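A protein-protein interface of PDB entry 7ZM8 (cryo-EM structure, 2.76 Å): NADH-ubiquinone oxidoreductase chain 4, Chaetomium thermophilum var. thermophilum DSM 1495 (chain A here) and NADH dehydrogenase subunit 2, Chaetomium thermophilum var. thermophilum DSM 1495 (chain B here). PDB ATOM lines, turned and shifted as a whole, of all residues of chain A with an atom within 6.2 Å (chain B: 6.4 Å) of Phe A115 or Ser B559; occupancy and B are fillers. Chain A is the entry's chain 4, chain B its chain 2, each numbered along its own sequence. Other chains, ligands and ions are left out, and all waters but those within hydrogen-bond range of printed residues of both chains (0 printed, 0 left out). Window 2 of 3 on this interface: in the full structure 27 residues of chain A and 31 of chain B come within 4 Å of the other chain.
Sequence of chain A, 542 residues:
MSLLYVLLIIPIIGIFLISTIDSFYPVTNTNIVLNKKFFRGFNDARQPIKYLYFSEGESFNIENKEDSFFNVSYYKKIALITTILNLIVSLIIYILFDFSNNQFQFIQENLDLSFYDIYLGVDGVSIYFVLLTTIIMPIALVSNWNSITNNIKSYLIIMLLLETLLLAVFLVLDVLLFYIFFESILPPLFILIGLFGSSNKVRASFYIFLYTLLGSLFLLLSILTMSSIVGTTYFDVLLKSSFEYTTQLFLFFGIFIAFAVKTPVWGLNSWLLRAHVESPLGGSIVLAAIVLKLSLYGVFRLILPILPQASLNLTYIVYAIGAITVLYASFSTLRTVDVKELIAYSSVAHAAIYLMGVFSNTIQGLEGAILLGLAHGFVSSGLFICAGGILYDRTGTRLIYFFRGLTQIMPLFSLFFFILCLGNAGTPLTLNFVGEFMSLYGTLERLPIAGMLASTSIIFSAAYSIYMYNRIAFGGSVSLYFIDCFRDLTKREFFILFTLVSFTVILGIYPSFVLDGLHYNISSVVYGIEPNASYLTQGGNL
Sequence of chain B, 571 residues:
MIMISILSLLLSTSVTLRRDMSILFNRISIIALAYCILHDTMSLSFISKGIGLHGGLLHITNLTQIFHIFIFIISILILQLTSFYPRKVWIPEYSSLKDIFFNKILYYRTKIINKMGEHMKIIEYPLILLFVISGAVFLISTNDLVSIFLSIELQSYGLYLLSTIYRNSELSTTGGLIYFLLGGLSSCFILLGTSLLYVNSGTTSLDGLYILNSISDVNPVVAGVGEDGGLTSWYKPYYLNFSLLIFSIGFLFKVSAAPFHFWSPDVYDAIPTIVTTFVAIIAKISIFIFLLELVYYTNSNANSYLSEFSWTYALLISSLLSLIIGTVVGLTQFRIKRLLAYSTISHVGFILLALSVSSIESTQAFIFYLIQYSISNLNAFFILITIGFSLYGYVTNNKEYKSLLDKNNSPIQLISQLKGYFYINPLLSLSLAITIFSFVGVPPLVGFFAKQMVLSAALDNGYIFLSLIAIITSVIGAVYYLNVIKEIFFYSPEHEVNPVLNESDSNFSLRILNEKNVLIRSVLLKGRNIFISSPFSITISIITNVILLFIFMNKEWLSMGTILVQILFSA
Hydrophobic or aromatic side chains of chain A that line the printed part of chain B: Phe A115 and Tyr A116. Hydrophobic or aromatic side chains of chain B that line the printed part of chain A: Leu B558. Among the printed residues, 9 pairs touch across the chains. Among the printed residues, no Asp or Glu carboxylate lies within 4 Å of a Lys or Arg side-chain nitrogen of the other chain.
The side-chain amide oxygen of Asn B554 is in hydrogen-bond range of the side-chain hydroxyl of Ser A114 (2.8 Å). N of Tyr A116 is in hydrogen-bond range of OD1 of Asn B554, at 3.4 Å.
The backbone carbonyl oxygen of Lys B555 is in hydrogen-bond range of the side-chain hydroxyl of Ser B559 (2.8 Å). OD2 of Asp A117 is in hydrogen-bond range of N of Ser A114.
Of chain B, only Asn B554, Lys B555, Leu B558 and Ser B559 come within 4 Å of Phe A115. Ser B559 touches one residue of chain A. Printed residues of chain A within 4 Å of Asn B554: Ser A114 (2.8 Å), Phe A115 (3.6 Å) and Tyr A116 (3.4 Å). Of the printed residues of chain A, Lys B555 touches Leu A113, Ser A114 and Phe A115. Of the printed residues of chain B, Ser A114 touches Asn B554 (2.8 Å) and Lys B555 (3.5 Å). Of the printed residues of chain B, Tyr A116 touches Asn B554 and Leu B558. Asp A117 touches none of the printed residues of chain B. The nearest printed residue of chain A that does not touch Ser B559 is Ser A114 (6.7 Å).
Leu A113 touches Lys B555 (O to CE, 3.5 Å). Lys B555 touches Ser A114 (CB to OG, 3.5 Å). Asn B554 touches Phe A115. Phe A115 touches Lys B555 (CE1 to O, 3.4 Å). Phe A115 touches Leu B558. Phe A115 touches Ser B559 (CE1 to OG, 3.3 Å). Leu B558 touches Tyr A116 (CD1 to CE2, 3.7 Å).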
ATOM      1  N   LEU A 113     -12.737  16.092 -14.515  1.00  0.00           N
ATOM      2  CA  LEU A 113     -12.922  17.445 -15.106  1.00  0.00           C
ATOM      3  C   LEU A 113     -14.198  17.522 -15.947  1.00  0.00           C
ATOM      4  O   LEU A 113     -14.428  16.612 -16.760  1.00  0.00           O
ATOM      5  CB  LEU A 113     -11.684  17.803 -15.934  1.00  0.00           C
ATOM      6  CG  LEU A 113     -10.711  18.782 -15.277  1.00  0.00           C
ATOM      7  CD1 LEU A 113     -10.314  18.322 -13.883  1.00  0.00           C
ATOM      8  CD2 LEU A 113      -9.476  18.981 -16.141  1.00  0.00           C
ATOM      9  N   SER A 114     -14.999  18.568 -15.738  1.00  0.00           N
ATOM     10  CA  SER A 114     -16.216  18.788 -16.560  1.00  0.00           C
ATOM     11  C   SER A 114     -16.092  20.164 -17.206  1.00  0.00           C
ATOM     12  O   SER A 114     -15.032  20.785 -17.050  1.00  0.00           O
ATOM     13  CB  SER A 114     -17.453  18.712 -15.714  1.00  0.00           C
ATOM     14  OG  SER A 114     -18.626  18.777 -16.509  1.00  0.00           O
ATOM     15  N   PHE A 115     -17.129  20.614 -17.906  1.00  0.00           N
ATOM     16  CA  PHE A 115     -17.143  21.977 -18.489  1.00  0.00           C
ATOM     17  C   PHE A 115     -17.122  23.021 -17.365  1.00  0.00           C
ATOM     18  O   PHE A 115     -16.317  23.949 -17.452  1.00  0.00           O
ATOM     19  CB  PHE A 115     -18.281  22.050 -19.502  1.00  0.00           C
ATOM     20  CG  PHE A 115     -18.237  20.971 -20.555  1.00  0.00           C
ATOM     21  CD1 PHE A 115     -18.764  19.712 -20.312  1.00  0.00           C
ATOM     22  CD2 PHE A 115     -17.668  21.213 -21.793  1.00  0.00           C
ATOM     23  CE1 PHE A 115     -18.711  18.722 -21.277  1.00  0.00           C
ATOM     24  CE2 PHE A 115     -17.623  20.222 -22.760  1.00  0.00           C
ATOM     25  CZ  PHE A 115     -18.145  18.980 -22.500  1.00  0.00           C
ATOM     26  N   TYR A 116     -17.935  22.848 -16.325  1.00  0.00           N
ATOM     27  CA  TYR A 116     -17.974  23.768 -15.163  1.00  0.00           C
ATOM     28  C   TYR A 116     -17.834  22.933 -13.897  1.00  0.00           C
ATOM     29  O   TYR A 116     -18.663  22.046 -13.698  1.00  0.00           O
ATOM     30  CB  TYR A 116     -19.278  24.563 -15.174  1.00  0.00           C
ATOM     31  CG  TYR A 116     -19.627  25.118 -16.529  1.00  0.00           C
ATOM     32  CD1 TYR A 116     -18.894  26.154 -17.084  1.00  0.00           C
ATOM     33  CD2 TYR A 116     -20.661  24.582 -17.274  1.00  0.00           C
ATOM     34  CE1 TYR A 116     -19.185  26.649 -18.343  1.00  0.00           C
ATOM     35  CE2 TYR A 116     -20.967  25.068 -18.532  1.00  0.00           C
ATOM     36  CZ  TYR A 116     -20.228  26.105 -19.067  1.00  0.00           C
ATOM     37  OH  TYR A 116     -20.535  26.591 -20.301  1.00  0.00           O
ATOM     38  N   ASP A 117     -16.824  23.198 -13.066  1.00  0.00           N
ATOM     39  CA  ASP A 117     -16.554  22.380 -11.851  1.00  0.00           C
ATOM     40  C   ASP A 117     -16.156  23.307 -10.706  1.00  0.00           C
ATOM     41  O   ASP A 117     -15.354  24.211 -10.947  1.00  0.00           O
ATOM     42  CB  ASP A 117     -15.413  21.398 -12.104  1.00  0.00           C
ATOM     43  CG  ASP A 117     -15.864  20.015 -12.536  1.00  0.00           C
ATOM     44  OD1 ASP A 117     -17.051  19.693 -12.336  1.00  0.00           O
ATOM     45  OD2 ASP A 117     -15.019  19.275 -13.062  1.00  0.00           O
ATOM     46  N   ASN B 554     -23.619  18.733 -15.752  1.00  0.00           N
ATOM     47  CA  ASN B 554     -23.440  19.314 -17.108  1.00  0.00           C
ATOM     48  C   ASN B 554     -22.589  18.452 -18.050  1.00  0.00           C
ATOM     49  O   ASN B 554     -22.674  18.704 -19.253  1.00  0.00           O
ATOM     50  CB  ASN B 554     -22.939  20.759 -16.986  1.00  0.00           C
ATOM     51  CG  ASN B 554     -21.627  20.897 -16.246  1.00  0.00           C
ATOM     52  OD1 ASN B 554     -20.562  20.799 -16.842  1.00  0.00           O
ATOM     53  ND2 ASN B 554     -21.693  21.142 -14.949  1.00  0.00           N
ATOM     54  N   LYS B 555     -21.856  17.458 -17.557  1.00  0.00           N
ATOM     55  CA  LYS B 555     -20.891  16.733 -18.439  1.00  0.00           C
ATOM     56  C   LYS B 555     -21.505  16.039 -19.661  1.00  0.00           C
ATOM     57  O   LYS B 555     -21.020  16.315 -20.751  1.00  0.00           O
ATOM     58  CB  LYS B 555     -20.024  15.743 -17.659  1.00  0.00           C
ATOM     59  CG  LYS B 555     -18.697  15.393 -18.315  1.00  0.00           C
ATOM     60  CD  LYS B 555     -17.888  14.390 -17.526  1.00  0.00           C
ATOM     61  CE  LYS B 555     -16.497  14.182 -18.087  1.00  0.00           C
ATOM     62  NZ  LYS B 555     -16.532  13.824 -19.524  1.00  0.00           N
ATOM     63  N   GLU B 556     -22.561  15.242 -19.517  1.00  0.00           N
ATOM     64  CA  GLU B 556     -23.024  14.401 -20.646  1.00  0.00           C
ATOM     65  C   GLU B 556     -23.897  15.193 -21.619  1.00  0.00           C
ATOM     66  O   GLU B 556     -23.912  14.831 -22.795  1.00  0.00           O
ATOM     67  CB  GLU B 556     -23.673  13.133 -20.088  1.00  0.00           C
ATOM     68  CG  GLU B 556     -22.725  12.249 -19.306  1.00  0.00           C
ATOM     69  CD  GLU B 556     -22.530  12.662 -17.859  1.00  0.00           C
ATOM     70  OE1 GLU B 556     -21.608  12.144 -17.215  1.00  0.00           O
ATOM     71  OE2 GLU B 556     -23.303  13.505 -17.385  1.00  0.00           O
ATOM     72  N   TRP B 557     -24.594  16.218 -21.145  1.00  0.00           N
ATOM     73  CA  TRP B 557     -25.398  17.114 -22.011  1.00  0.00           C
ATOM     74  C   TRP B 557     -24.467  17.900 -22.944  1.00  0.00           C
ATOM     75  O   TRP B 557     -24.755  17.966 -24.155  1.00  0.00           O
ATOM     76  CB  TRP B 557     -26.273  18.009 -21.117  1.00  0.00           C
ATOM     77  CG  TRP B 557     -27.333  18.856 -21.755  1.00  0.00           C
ATOM     78  CD1 TRP B 557     -27.535  19.087 -23.081  1.00  0.00           C
ATOM     79  CD2 TRP B 557     -28.345  19.609 -21.066  1.00  0.00           C
ATOM     80  NE1 TRP B 557     -28.597  19.929 -23.265  1.00  0.00           N
ATOM     81  CE2 TRP B 557     -29.118  20.263 -22.046  1.00  0.00           C
ATOM     82  CE3 TRP B 557     -28.680  19.795 -19.721  1.00  0.00           C
ATOM     83  CZ2 TRP B 557     -30.196  21.083 -21.722  1.00  0.00           C
ATOM     84  CZ3 TRP B 557     -29.748  20.603 -19.399  1.00  0.00           C
ATOM     85  CH2 TRP B 557     -30.491  21.241 -20.389  1.00  0.00           C
ATOM     86  N   LEU B 558     -23.395  18.475 -22.406  1.00  0.00           N
ATOM     87  CA  LEU B 558     -22.503  19.313 -23.243  1.00  0.00           C
ATOM     88  C   LEU B 558     -21.537  18.436 -24.037  1.00  0.00           C
ATOM     89  O   LEU B 558     -21.135  18.860 -25.119  1.00  0.00           O
ATOM     90  CB  LEU B 558     -21.805  20.330 -22.341  1.00  0.00           C
ATOM     91  CG  LEU B 558     -22.713  21.383 -21.714  1.00  0.00           C
ATOM     92  CD1 LEU B 558     -21.987  22.132 -20.610  1.00  0.00           C
ATOM     93  CD2 LEU B 558     -23.225  22.347 -22.771  1.00  0.00           C
ATOM     94  N   SER B 559     -21.190  17.261 -23.516  1.00  0.00           N
ATOM     95  CA  SER B 559     -20.316  16.285 -24.223  1.00  0.00           C
ATOM     96  C   SER B 559     -21.004  15.772 -25.486  1.00  0.00           C
ATOM     97  O   SER B 559     -20.309  15.513 -26.460  1.00  0.00           O
ATOM     98  CB  SER B 559     -19.905  15.160 -23.321  1.00  0.00           C
ATOM     99  OG  SER B 559     -18.929  15.579 -22.383  1.00  0.00           O
ATOM    100  N   MET B 560     -22.318  15.581 -25.436  1.00  0.00           N
ATOM    101  CA  MET B 560     -23.085  15.104 -26.603  1.00  0.00           C
ATOM    102  C   MET B 560     -22.961  16.124 -27.719  1.00  0.00           C
ATOM    103  O   MET B 560     -22.684  15.716 -28.843  1.00  0.00           O
ATOM    104  CB  MET B 560     -24.552  15.032 -26.180  1.00  0.00           C
ATOM    105  CG  MET B 560     -25.515  14.689 -27.291  1.00  0.00           C
ATOM    106  SD  MET B 560     -27.188  15.163 -26.815  1.00  0.00           S
ATOM    107  CE  MET B 560     -27.136  16.925 -27.141  1.00  0.00           C
ATOM    108  N   GLY B 561     -23.141  17.400 -27.402  1.00  0.00           N
ATOM    109  CA  GLY B 561     -22.990  18.483 -28.384  1.00  0.00           C
ATOM    110  C   GLY B 561     -21.571  18.649 -28.878  1.00  0.00           C
ATOM    111  O   GLY B 561     -21.421  18.947 -30.060  1.00  0.00           O
ATOM    112  N   THR B 562     -20.568  18.492 -28.013  1.00  0.00           N
ATOM    113  CA  THR B 562     -19.168  18.555 -28.498  1.00  0.00           C
ATOM    114  C   THR B 562     -18.923  17.442 -29.514  1.00  0.00           C
ATOM    115  O   THR B 562     -18.331  17.755 -30.539  1.00  0.00           O
ATOM    116  CB  THR B 562     -18.112  18.712 -27.392  1.00  0.00           C
ATOM    117  OG1 THR B 562     -16.849  18.868 -28.036  1.00  0.00           O
ATOM    118  CG2 THR B 562     -18.006  17.539 -26.449  1.00  0.00           C
ATOM    119  N   ILE B 563     -19.435  16.238 -29.268  1.00  0.00           N
ATOM    120  CA  ILE B 563     -19.287  15.102 -30.221  1.00  0.00           C
ATOM    121  C   ILE B 563     -20.116  15.352 -31.487  1.00  0.00           C
ATOM    122  O   ILE B 563     -19.599  15.065 -32.575  1.00  0.00           O
ATOM    123  CB  ILE B 563     -19.647  13.775 -29.538  1.00  0.00           C
ATOM    124  CG1 ILE B 563     -18.703  13.458 -28.378  1.00  0.00           C
ATOM    125  CG2 ILE B 563     -19.697  12.637 -30.540  1.00  0.00           C
ATOM    126  CD1 ILE B 563     -19.091  12.237 -27.589  1.00  0.00           C
ATOM    127  N   LEU B 564     -21.337  15.877 -31.377  1.00  0.00           N
ATOM    128  CA  LEU B 564     -22.165  16.018 -32.602  1.00  0.00           C
ATOM    129  C   LEU B 564     -21.491  17.007 -33.546  1.00  0.00           C
ATOM    130  O   LEU B 564     -21.436  16.720 -34.751  1.00  0.00           O
ATOM    131  CB  LEU B 564     -23.606  16.426 -32.265  1.00  0.00           C
ATOM    132  CG  LEU B 564     -24.452  15.385 -31.538  1.00  0.00           C
ATOM    133  CD1 LEU B 564     -25.800  15.967 -31.149  1.00  0.00           C
ATOM    134  CD2 LEU B 564     -24.631  14.144 -32.392  1.00  0.00           C
